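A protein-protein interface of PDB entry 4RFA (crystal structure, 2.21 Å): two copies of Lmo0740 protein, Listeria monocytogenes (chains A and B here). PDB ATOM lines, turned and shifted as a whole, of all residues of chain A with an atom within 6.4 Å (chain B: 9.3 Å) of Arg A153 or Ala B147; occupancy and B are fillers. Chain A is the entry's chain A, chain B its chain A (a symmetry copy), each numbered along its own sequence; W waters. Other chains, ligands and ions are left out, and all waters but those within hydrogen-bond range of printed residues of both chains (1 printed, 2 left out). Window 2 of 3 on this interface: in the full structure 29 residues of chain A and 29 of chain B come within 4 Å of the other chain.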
ATOM      1  N   TYR A  71     -20.577 -26.641  13.382  1.00  0.00           N
ATOM      2  CA  TYR A  71     -20.956 -26.771  14.761  1.00  0.00           C
ATOM      3  C   TYR A  71     -22.179 -25.918  15.021  1.00  0.00           C
ATOM      4  O   TYR A  71     -22.477 -24.977  14.300  1.00  0.00           O
ATOM      5  CB  TYR A  71     -19.814 -26.280  15.642  1.00  0.00           C
ATOM      6  CG  TYR A  71     -18.561 -27.127  15.597  1.00  0.00           C
ATOM      7  CD1 TYR A  71     -18.621 -28.494  15.362  1.00  0.00           C
ATOM      8  CD2 TYR A  71     -17.308 -26.556  15.841  1.00  0.00           C
ATOM      9  CE1 TYR A  71     -17.472 -29.276  15.353  1.00  0.00           C
ATOM     10  CE2 TYR A  71     -16.146 -27.332  15.844  1.00  0.00           C
ATOM     11  CZ  TYR A  71     -16.236 -28.695  15.596  1.00  0.00           C
ATOM     12  OH  TYR A  71     -15.102 -29.482  15.590  1.00  0.00           O
ATOM     13  N   MET A 145     -18.209 -24.292  28.902  1.00  0.00           N
ATOM     14  CA  MET A 145     -17.687 -25.385  28.096  1.00  0.00           C
ATOM     15  C   MET A 145     -16.278 -25.122  27.635  1.00  0.00           C
ATOM     16  O   MET A 145     -15.592 -26.060  27.172  1.00  0.00           O
ATOM     17  CB  MET A 145     -18.583 -25.582  26.877  1.00  0.00           C
ATOM     18  CG  MET A 145     -19.703 -26.570  27.177  1.00  0.00           C
ATOM     19  SD  MET A 145     -20.559 -27.123  25.491  1.00  0.00           S
ATOM     20  CE  MET A 145     -21.914 -28.331  26.254  1.00  0.00           C
ATOM     21  N   ILE A 146     -15.831 -23.876  27.745  1.00  0.00           N
ATOM     22  CA  ILE A 146     -14.468 -23.466  27.299  1.00  0.00           C
ATOM     23  C   ILE A 146     -13.420 -24.221  28.088  1.00  0.00           C
ATOM     24  O   ILE A 146     -13.592 -24.446  29.263  1.00  0.00           O
ATOM     25  CB  ILE A 146     -14.286 -21.943  27.431  1.00  0.00           C
ATOM     26  CG1 ILE A 146     -15.203 -21.219  26.478  1.00  0.00           C
ATOM     27  CG2 ILE A 146     -12.845 -21.518  27.134  1.00  0.00           C
ATOM     28  CD1 ILE A 146     -15.236 -19.717  26.650  1.00  0.00           C
ATOM     29  N   ALA A 147     -12.370 -24.687  27.413  1.00  0.00           N
ATOM     30  CA  ALA A 147     -11.305 -25.456  28.087  1.00  0.00           C
ATOM     31  C   ALA A 147     -11.719 -26.815  28.667  1.00  0.00           C
ATOM     32  O   ALA A 147     -11.123 -27.274  29.632  1.00  0.00           O
ATOM     33  CB  ALA A 147     -10.638 -24.594  29.192  1.00  0.00           C
ATOM     34  N   LYS A 148     -12.772 -27.443  28.150  1.00  0.00           N
ATOM     35  CA  LYS A 148     -13.173 -28.741  28.655  1.00  0.00           C
ATOM     36  C   LYS A 148     -12.911 -29.793  27.606  1.00  0.00           C
ATOM     37  O   LYS A 148     -12.904 -29.511  26.399  1.00  0.00           O
ATOM     38  CB  LYS A 148     -14.657 -28.763  28.984  1.00  0.00           C
ATOM     39  CG  LYS A 148     -15.148 -27.824  30.052  1.00  0.00           C
ATOM     40  CD  LYS A 148     -14.525 -28.005  31.403  1.00  0.00           C
ATOM     41  CE  LYS A 148     -15.320 -27.116  32.369  1.00  0.00           C
ATOM     42  NZ  LYS A 148     -14.868 -27.360  33.753  1.00  0.00           N
ATOM     43  N   THR A 149     -12.730 -31.017  28.061  1.00  0.00           N
ATOM     44  CA  THR A 149     -12.567 -32.165  27.178  1.00  0.00           C
ATOM     45  C   THR A 149     -13.925 -32.507  26.520  1.00  0.00           C
ATOM     46  O   THR A 149     -14.968 -32.073  26.960  1.00  0.00           O
ATOM     47  CB  THR A 149     -12.150 -33.407  27.965  1.00  0.00           C
ATOM     48  OG1 THR A 149     -13.166 -33.683  28.935  1.00  0.00           O
ATOM     49  CG2 THR A 149     -10.836 -33.176  28.703  1.00  0.00           C
ATOM     50  N   PRO A 150     -13.900 -33.307  25.468  1.00  0.00           N
ATOM     51  CA  PRO A 150     -15.192 -33.654  24.888  1.00  0.00           C
ATOM     52  C   PRO A 150     -16.123 -34.367  25.851  1.00  0.00           C
ATOM     53  O   PRO A 150     -17.315 -34.120  25.829  1.00  0.00           O
ATOM     54  CB  PRO A 150     -14.811 -34.539  23.700  1.00  0.00           C
ATOM     55  CG  PRO A 150     -13.467 -34.004  23.280  1.00  0.00           C
ATOM     56  CD  PRO A 150     -12.771 -33.681  24.588  1.00  0.00           C
ATOM     57  N   LYS A 151     -15.574 -35.176  26.733  1.00  0.00           N
ATOM     58  CA  LYS A 151     -16.384 -35.887  27.718  1.00  0.00           C
ATOM     59  C   LYS A 151     -17.047 -34.955  28.686  1.00  0.00           C
ATOM     60  O   LYS A 151     -18.219 -35.093  29.035  1.00  0.00           O
ATOM     61  CB  LYS A 151     -15.510 -36.880  28.502  1.00  0.00           C
ATOM     62  CG  LYS A 151     -16.229 -37.595  29.653  1.00  0.00           C
ATOM     63  CD  LYS A 151     -16.795 -38.943  29.245  1.00  0.00           C
ATOM     64  CE  LYS A 151     -17.483 -39.672  30.401  1.00  0.00           C
ATOM     65  NZ  LYS A 151     -16.558 -40.419  31.268  1.00  0.00           N
ATOM     66  N   GLU A 152     -16.288 -34.010  29.184  1.00  0.00           N
ATOM     67  CA  GLU A 152     -16.901 -33.010  30.029  1.00  0.00           C
ATOM     68  C   GLU A 152     -17.946 -32.219  29.292  1.00  0.00           C
ATOM     69  O   GLU A 152     -18.954 -31.872  29.862  1.00  0.00           O
ATOM     70  CB  GLU A 152     -15.835 -32.072  30.548  1.00  0.00           C
ATOM     71  CG  GLU A 152     -14.847 -32.768  31.469  1.00  0.00           C
ATOM     72  CD  GLU A 152     -13.715 -31.847  31.806  1.00  0.00           C
ATOM     73  OE1 GLU A 152     -13.080 -31.300  30.865  1.00  0.00           O
ATOM     74  OE2 GLU A 152     -13.520 -31.622  33.001  1.00  0.00           O
ATOM     75  N   ARG A 153     -17.702 -31.898  28.026  1.00  0.00           N
ATOM     76  CA  ARG A 153     -18.685 -31.148  27.260  1.00  0.00           C
ATOM     77  C   ARG A 153     -20.005 -31.881  27.049  1.00  0.00           C
ATOM     78  O   ARG A 153     -21.071 -31.275  27.081  1.00  0.00           O
ATOM     79  CB  ARG A 153     -18.108 -30.775  25.908  1.00  0.00           C
ATOM     80  CG  ARG A 153     -16.988 -29.766  26.035  1.00  0.00           C
ATOM     81  CD  ARG A 153     -16.705 -28.973  24.793  1.00  0.00           C
ATOM     82  NE  ARG A 153     -16.360 -29.757  23.604  1.00  0.00           N
ATOM     83  CZ  ARG A 153     -15.134 -30.122  23.236  1.00  0.00           C
ATOM     84  NH1 ARG A 153     -14.061 -29.862  24.003  1.00  0.00           N
ATOM     85  NH2 ARG A 153     -14.978 -30.755  22.080  1.00  0.00           N
ATOM     86  N   ILE A 154     -19.949 -33.193  26.839  1.00  0.00           N
ATOM     87  CA  ILE A 154     -21.175 -33.927  26.541  1.00  0.00           C
ATOM     88  C   ILE A 154     -22.102 -33.975  27.754  1.00  0.00           C
ATOM     89  O   ILE A 154     -23.330 -33.862  27.628  1.00  0.00           O
ATOM     90  CB  ILE A 154     -20.867 -35.331  25.973  1.00  0.00           C
ATOM     91  CG1 ILE A 154     -22.141 -35.954  25.399  1.00  0.00           C
ATOM     92  CG2 ILE A 154     -20.241 -36.261  27.006  1.00  0.00           C
ATOM     93  CD1 ILE A 154     -21.880 -37.254  24.692  1.00  0.00           C
ATOM     94  N   TYR A 155     -21.536 -34.130  28.943  1.00  0.00           N
ATOM     95  CA  TYR A 155     -22.371 -34.031  30.152  1.00  0.00           C
ATOM     96  C   TYR A 155     -23.045 -32.693  30.243  1.00  0.00           C
ATOM     97  O   TYR A 155     -24.220 -32.608  30.555  1.00  0.00           O
ATOM     98  CB  TYR A 155     -21.498 -34.216  31.397  1.00  0.00           C
ATOM     99  CG  TYR A 155     -21.390 -35.676  31.872  1.00  0.00           C
ATOM    100  CD1 TYR A 155     -22.452 -36.265  32.527  1.00  0.00           C
ATOM    101  CD2 TYR A 155     -20.241 -36.426  31.694  1.00  0.00           C
ATOM    102  CE1 TYR A 155     -22.395 -37.569  33.004  1.00  0.00           C
ATOM    103  CE2 TYR A 155     -20.155 -37.729  32.187  1.00  0.00           C
ATOM    104  CZ  TYR A 155     -21.260 -38.294  32.817  1.00  0.00           C
ATOM    105  OH  TYR A 155     -21.279 -39.567  33.313  1.00  0.00           O
ATOM    106  N   MET A 156     -22.265 -31.629  30.037  1.00  0.00           N
ATOM    107  CA  MET A 156     -22.756 -30.274  30.188  1.00  0.00           C
ATOM    108  C   MET A 156     -23.766 -30.017  29.117  1.00  0.00           C
ATOM    109  O   MET A 156     -24.773 -29.415  29.411  1.00  0.00           O
ATOM    110  CB  MET A 156     -21.665 -29.190  30.042  1.00  0.00           C
ATOM    111  CG  MET A 156     -20.721 -29.274  31.231  1.00  0.00           C
ATOM    112  SD  MET A 156     -19.112 -28.135  30.928  1.00  0.00           S
ATOM    113  CE  MET A 156     -20.145 -26.486  31.103  1.00  0.00           C
ATOM    114  N   ALA A 157     -23.500 -30.436  27.875  1.00  0.00           N
ATOM    115  CA  ALA A 157     -24.508 -30.306  26.823  1.00  0.00           C
ATOM    116  C   ALA A 157     -25.846 -30.993  27.203  1.00  0.00           C
ATOM    117  O   ALA A 157     -26.927 -30.434  27.064  1.00  0.00           O
ATOM    118  CB  ALA A 157     -23.983 -30.879  25.521  1.00  0.00           C
ATOM    119  N   LEU A 158     -25.785 -32.255  27.581  1.00  0.00           N
ATOM    120  CA  LEU A 158     -27.007 -33.002  27.799  1.00  0.00           C
ATOM    121  C   LEU A 158     -27.752 -32.429  28.967  1.00  0.00           C
ATOM    122  O   LEU A 158     -28.988 -32.420  28.975  1.00  0.00           O
ATOM    123  CB  LEU A 158     -26.697 -34.465  28.060  1.00  0.00           C
ATOM    124  CG  LEU A 158     -26.354 -35.240  26.802  1.00  0.00           C
ATOM    125  CD1 LEU A 158     -25.807 -36.609  27.159  1.00  0.00           C
ATOM    126  CD2 LEU A 158     -27.551 -35.351  25.856  1.00  0.00           C
ATOM    127  N   TYR A 189     -23.229 -29.835  18.578  1.00  0.00           N
ATOM    128  CA  TYR A 189     -23.411 -28.935  19.710  1.00  0.00           C
ATOM    129  C   TYR A 189     -22.261 -29.069  20.695  1.00  0.00           C
ATOM    130  O   TYR A 189     -21.885 -28.099  21.399  1.00  0.00           O
ATOM    131  CB  TYR A 189     -24.753 -29.191  20.337  1.00  0.00           C
ATOM    132  CG  TYR A 189     -25.120 -28.371  21.568  1.00  0.00           C
ATOM    133  CD1 TYR A 189     -25.296 -27.001  21.528  1.00  0.00           C
ATOM    134  CD2 TYR A 189     -25.407 -29.022  22.764  1.00  0.00           C
ATOM    135  CE1 TYR A 189     -25.718 -26.283  22.652  1.00  0.00           C
ATOM    136  CE2 TYR A 189     -25.812 -28.312  23.889  1.00  0.00           C
ATOM    137  CZ  TYR A 189     -25.959 -26.947  23.828  1.00  0.00           C
ATOM    138  OH  TYR A 189     -26.325 -26.343  24.991  1.00  0.00           O
ATOM    139  N   CYS A 190     -21.719 -30.282  20.787  1.00  0.00           N
ATOM    140  CA  CYS A 190     -20.539 -30.534  21.618  1.00  0.00           C
ATOM    141  C   CYS A 190     -19.223 -30.162  20.966  1.00  0.00           C
ATOM    142  O   CYS A 190     -18.184 -30.285  21.588  1.00  0.00           O
ATOM    143  CB  CYS A 190     -20.475 -31.990  22.102  1.00  0.00           C
ATOM    144  SG  CYS A 190     -21.848 -32.379  23.186  1.00  0.00           S
ATOM    145  N   ARG A 191     -19.298 -29.751  19.712  1.00  0.00           N
ATOM    146  CA  ARG A 191     -18.143 -29.321  18.965  1.00  0.00           C
ATOM    147  C   ARG A 191     -17.060 -30.448  19.023  1.00  0.00           C
ATOM    148  O   ARG A 191     -15.938 -30.280  19.524  1.00  0.00           O
ATOM    149  CB  ARG A 191     -17.747 -27.912  19.480  1.00  0.00           C
ATOM    150  CG  ARG A 191     -18.964 -26.934  19.642  1.00  0.00           C
ATOM    151  CD  ARG A 191     -18.494 -25.505  19.947  1.00  0.00           C
ATOM    152  NE  ARG A 191     -19.399 -24.382  20.367  1.00  0.00           N
ATOM    153  CZ  ARG A 191     -20.634 -24.391  20.890  1.00  0.00           C
ATOM    154  NH1 ARG A 191     -21.309 -25.499  21.134  1.00  0.00           N
ATOM    155  NH2 ARG A 191     -21.184 -23.187  21.226  1.00  0.00           N
ATOM    156  N   THR A 192     -17.485 -31.634  18.586  1.00  0.00           N
ATOM    157  CA  THR A 192     -16.626 -32.794  18.388  1.00  0.00           C
ATOM    158  C   THR A 192     -17.160 -33.688  17.232  1.00  0.00           C
ATOM    159  O   THR A 192     -18.090 -33.314  16.553  1.00  0.00           O
ATOM    160  CB  THR A 192     -16.539 -33.612  19.659  1.00  0.00           C
ATOM    161  OG1 THR A 192     -15.471 -34.523  19.527  1.00  0.00           O
ATOM    162  CG2 THR A 192     -17.837 -34.366  19.955  1.00  0.00           C
ATOM    163  N   ASN A 196     -16.585 -39.897  17.934  1.00  0.00           N
ATOM    164  CA  ASN A 196     -16.246 -39.617  19.306  1.00  0.00           C
ATOM    165  C   ASN A 196     -17.495 -39.519  20.179  1.00  0.00           C
ATOM    166  O   ASN A 196     -17.546 -40.062  21.266  1.00  0.00           O
ATOM    167  CB  ASN A 196     -15.431 -38.340  19.374  1.00  0.00           C
ATOM    168  CG  ASN A 196     -14.685 -38.217  20.662  1.00  0.00           C
ATOM    169  OD1 ASN A 196     -14.422 -39.215  21.322  1.00  0.00           O
ATOM    170  ND2 ASN A 196     -14.356 -36.999  21.044  1.00  0.00           N
ATOM    171  N   LEU B 142     -16.940 -15.155  22.351  1.00  0.00           N
ATOM    172  CA  LEU B 142     -16.393 -16.034  23.357  1.00  0.00           C
ATOM    173  C   LEU B 142     -16.734 -17.459  23.144  1.00  0.00           C
ATOM    174  O   LEU B 142     -15.874 -18.351  23.406  1.00  0.00           O
ATOM    175  CB  LEU B 142     -16.816 -15.632  24.763  1.00  0.00           C
ATOM    176  CG  LEU B 142     -16.067 -14.368  25.144  1.00  0.00           C
ATOM    177  CD1 LEU B 142     -16.758 -13.744  26.325  1.00  0.00           C
ATOM    178  CD2 LEU B 142     -14.647 -14.688  25.499  1.00  0.00           C
ATOM    179  N   LEU B 143     -17.964 -17.717  22.726  1.00  0.00           N
ATOM    180  CA  LEU B 143     -18.346 -19.111  22.420  1.00  0.00           C
ATOM    181  C   LEU B 143     -17.400 -19.740  21.372  1.00  0.00           C
ATOM    182  O   LEU B 143     -17.178 -20.955  21.348  1.00  0.00           O
ATOM    183  CB  LEU B 143     -19.795 -19.201  21.958  1.00  0.00           C
ATOM    184  CG  LEU B 143     -20.889 -18.874  23.007  1.00  0.00           C
ATOM    185  CD1 LEU B 143     -22.252 -18.879  22.333  1.00  0.00           C
ATOM    186  CD2 LEU B 143     -20.907 -19.889  24.125  1.00  0.00           C
ATOM    187  N   GLY B 144     -16.825 -18.926  20.512  1.00  0.00           N
ATOM    188  CA  GLY B 144     -15.851 -19.447  19.536  1.00  0.00           C
ATOM    189  C   GLY B 144     -14.601 -20.061  20.162  1.00  0.00           C
ATOM    190  O   GLY B 144     -13.796 -20.715  19.473  1.00  0.00           O
ATOM    191  N   MET B 145     -14.442 -19.884  21.469  1.00  0.00           N
ATOM    192  CA  MET B 145     -13.278 -20.406  22.172  1.00  0.00           C
ATOM    193  C   MET B 145     -13.455 -21.851  22.557  1.00  0.00           C
ATOM    194  O   MET B 145     -12.463 -22.522  22.916  1.00  0.00           O
ATOM    195  CB  MET B 145     -13.040 -19.578  23.431  1.00  0.00           C
ATOM    196  CG  MET B 145     -12.119 -18.399  23.143  1.00  0.00           C
ATOM    197  SD  MET B 145     -11.494 -17.625  24.844  1.00  0.00           S
ATOM    198  CE  MET B 145     -10.392 -16.174  24.096  1.00  0.00           C
ATOM    199  N   ILE B 146     -14.686 -22.345  22.495  1.00  0.00           N
ATOM    200  CA  ILE B 146     -15.012 -23.749  22.877  1.00  0.00           C
ATOM    201  C   ILE B 146     -14.268 -24.713  21.978  1.00  0.00           C
ATOM    202  O   ILE B 146     -14.126 -24.459  20.804  1.00  0.00           O
ATOM    203  CB  ILE B 146     -16.532 -23.990  22.827  1.00  0.00           C
ATOM    204  CG1 ILE B 146     -17.229 -23.167  23.880  1.00  0.00           C
ATOM    205  CG2 ILE B 146     -16.878 -25.463  23.057  1.00  0.00           C
ATOM    206  CD1 ILE B 146     -18.740 -23.188  23.803  1.00  0.00           C
ATOM    207  N   ALA B 147     -13.718 -25.780  22.554  1.00  0.00           N
ATOM    208  CA  ALA B 147     -12.951 -26.767  21.767  1.00  0.00           C
ATOM    209  C   ALA B 147     -11.650 -26.259  21.132  1.00  0.00           C
ATOM    210  O   ALA B 147     -11.230 -26.773  20.104  1.00  0.00           O
ATOM    211  CB  ALA B 147     -13.855 -27.402  20.677  1.00  0.00           C
ATOM    212  N   LYS B 148     -11.033 -25.213  21.676  1.00  0.00           N
ATOM    213  CA  LYS B 148      -9.787 -24.725  21.120  1.00  0.00           C
ATOM    214  C   LYS B 148      -8.660 -25.004  22.083  1.00  0.00           C
ATOM    215  O   LYS B 148      -8.863 -25.097  23.301  1.00  0.00           O
ATOM    216  CB  LYS B 148      -9.845 -23.223  20.885  1.00  0.00           C
ATOM    217  CG  LYS B 148     -10.870 -22.710  19.911  1.00  0.00           C
ATOM    218  CD  LYS B 148     -10.752 -23.240  18.513  1.00  0.00           C
ATOM    219  CE  LYS B 148     -11.732 -22.427  17.657  1.00  0.00           C
ATOM    220  NZ  LYS B 148     -11.559 -22.782  16.235  1.00  0.00           N
ATOM    221  N   THR B 149      -7.461 -25.102  21.542  1.00  0.00           N
ATOM    222  CA  THR B 149      -6.254 -25.269  22.341  1.00  0.00           C
ATOM    223  C   THR B 149      -5.925 -23.940  23.062  1.00  0.00           C
ATOM    224  O   THR B 149      -6.429 -22.892  22.718  1.00  0.00           O
ATOM    225  CB  THR B 149      -5.050 -25.582  21.455  1.00  0.00           C
ATOM    226  OG1 THR B 149      -4.878 -24.497  20.536  1.00  0.00           O
ATOM    227  CG2 THR B 149      -5.274 -26.856  20.649  1.00  0.00           C
ATOM    228  N   PRO B 150      -5.059 -23.995  24.060  1.00  0.00           N
ATOM    229  CA  PRO B 150      -4.727 -22.727  24.699  1.00  0.00           C
ATOM    230  C   PRO B 150      -4.116 -21.708  23.756  1.00  0.00           C
ATOM    231  O   PRO B 150      -4.409 -20.531  23.869  1.00  0.00           O
ATOM    232  CB  PRO B 150      -3.753 -23.140  25.803  1.00  0.00           C
ATOM    233  CG  PRO B 150      -4.206 -24.529  26.168  1.00  0.00           C
ATOM    234  CD  PRO B 150      -4.584 -25.158  24.841  1.00  0.00           C
ATOM    235  N   GLU B 152      -4.692 -21.354  20.468  1.00  0.00           N
ATOM    236  CA  GLU B 152      -5.768 -20.734  19.727  1.00  0.00           C
ATOM    237  C   GLU B 152      -6.552 -19.773  20.577  1.00  0.00           C
ATOM    238  O   GLU B 152      -6.974 -18.748  20.095  1.00  0.00           O
ATOM    239  CB  GLU B 152      -6.694 -21.807  19.199  1.00  0.00           C
ATOM    240  CG  GLU B 152      -6.019 -22.705  18.176  1.00  0.00           C
ATOM    241  CD  GLU B 152      -6.914 -23.854  17.825  1.00  0.00           C
ATOM    242  OE1 GLU B 152      -7.373 -24.569  18.755  1.00  0.00           O
ATOM    243  OE2 GLU B 152      -7.206 -23.984  16.635  1.00  0.00           O
ATOM    244  N   ARG B 153      -6.781 -20.108  21.841  1.00  0.00           N
ATOM    245  CA  ARG B 153      -7.519 -19.207  22.714  1.00  0.00           C
ATOM    246  C   ARG B 153      -6.827 -17.873  22.963  1.00  0.00           C
ATOM    247  O   ARG B 153      -7.476 -16.834  23.037  1.00  0.00           O
ATOM    248  CB  ARG B 153      -7.781 -19.883  24.046  1.00  0.00           C
ATOM    249  CG  ARG B 153      -8.750 -21.036  23.910  1.00  0.00           C
ATOM    250  CD  ARG B 153      -9.450 -21.429  25.178  1.00  0.00           C
ATOM    251  NE  ARG B 153      -8.579 -21.812  26.293  1.00  0.00           N
ATOM    252  CZ  ARG B 153      -8.141 -23.041  26.557  1.00  0.00           C
ATOM    253  NH1 ARG B 153      -8.407 -24.076  25.741  1.00  0.00           N
ATOM    254  NH2 ARG B 153      -7.429 -23.240  27.660  1.00  0.00           N
ATOM    255  N   MET B 156      -7.361 -15.446  20.148  1.00  0.00           N
ATOM    256  CA  MET B 156      -8.741 -15.007  20.113  1.00  0.00           C
ATOM    257  C   MET B 156      -8.969 -14.077  21.260  1.00  0.00           C
ATOM    258  O   MET B 156      -9.628 -13.082  21.068  1.00  0.00           O
ATOM    259  CB  MET B 156      -9.769 -16.152  20.254  1.00  0.00           C
ATOM    260  CG  MET B 156      -9.723 -17.016  19.004  1.00  0.00           C
ATOM    261  SD  MET B 156     -10.775 -18.690  19.273  1.00  0.00           S
ATOM    262  CE  MET B 156     -12.473 -17.722  19.267  1.00  0.00           C
HETATM  263  O   HOH W   1     -10.934 -27.256  24.853  1.00  0.00           O
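The guanidinium group of Arg A153 lies within hydrogen-bond range of the backbone carbonyl oxygen of Lys A148 (2.7 Å). The guanidinium group (NE) of Arg A153 is in hydrogen-bond range of the backbone carbonyl oxygen (O) of Cys A190, at 2.8 Å. The guanidinium group (NH2) of Arg A153 lies within hydrogen-bond range of the backbone carbonyl oxygen (O) of Arg A191. O of Tyr A189 sits at hydrogen-bond distance from NH1 of Arg A191 (2.7 Å). The guanidinium group (NH1) of Arg B153 lies within hydrogen-bond range of the backbone carbonyl oxygen (O) of Lys B148 (2.7 Å).
Ile B146 touches Met A145 (CD1 to CB, 3.9 Å). Ile A146 touches Leu B142 (CD1 to O, 3.6 Å). Ile A146 touches Met B145 (CD1 to CB, 3.9 Å). Ile A146 touches Ile B146. CD of Arg B153 touches CG2 of Ile A146 (3.9 Å). Ala A147 touches Arg B153. CG2 of Ile B146 touches CD of Arg A153, at 3.9 Å. NH2 of Arg A153 touches CB of Ala B147, at 3.8 Å. Arg A191 touches Ile B146. Arg A191 touches Ala B147 (O to CB, 3.7 Å).
Arg A153 touches just these residues of chain B: Ile B146 and Ala B147. Of the printed residues of chain A, Ala B147 touches Arg A153 and Arg A191. Of the printed residues of chain B, Met A145 touches Ile B146. Of the printed residues of chain B, Arg A191 touches Ile B146 (3.5 Å) and Ala B147 (3.7 Å). The nearest residue of chain B that does not touch Arg A153 is Lys B148 (6.0 Å). The nearest printed residue of chain A that does not touch Ala B147 is Met A145 (5.0 Å). The nearest printed residue of chain B that does not touch Ile A146 is Leu B143 (5.2 Å).
Of the 12 printed residues of chain B, 5 touch a printed residue of chain A. Of the 20 printed residues of chain A, 5 touch a printed residue of chain B. Hydrophobic or aromatic side chains of chain A that line the printed part of chain B: Met A145, Ile A146 and Ala A147. Along chain A the printed residues that touch a printed residue of chain B span positions 145 to 191. Among the printed residues, no Asp or Glu carboxylate lies within 4 Å of a Lys or Arg side-chain nitrogen of the other chain.
Met A145 touches Ile B146, and with the chains exchanged Ile A146 touches Met B145. Ile A146 touches its own counterpart, Ile B146. Ile A146 touches Arg B153, and with the chains exchanged Arg A153 touches Ile B146. Ala A147 touches Arg B153, and with the chains exchanged Arg A153 touches Ala B147. Positions printed for both chains: 145, 146, 147, 148, 149, 150, 152, 153 and 156. Of the 10 pairs that touch across the chains among the printed residues, 7 have their exchanged pair printed and touching as well.
Water W1 lies within hydrogen-bond range of the backbone carbonyl oxygen of Lys B148 (3.4 Å) and the backbone carbonyl oxygen of Lys A148 (3.4 Å).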
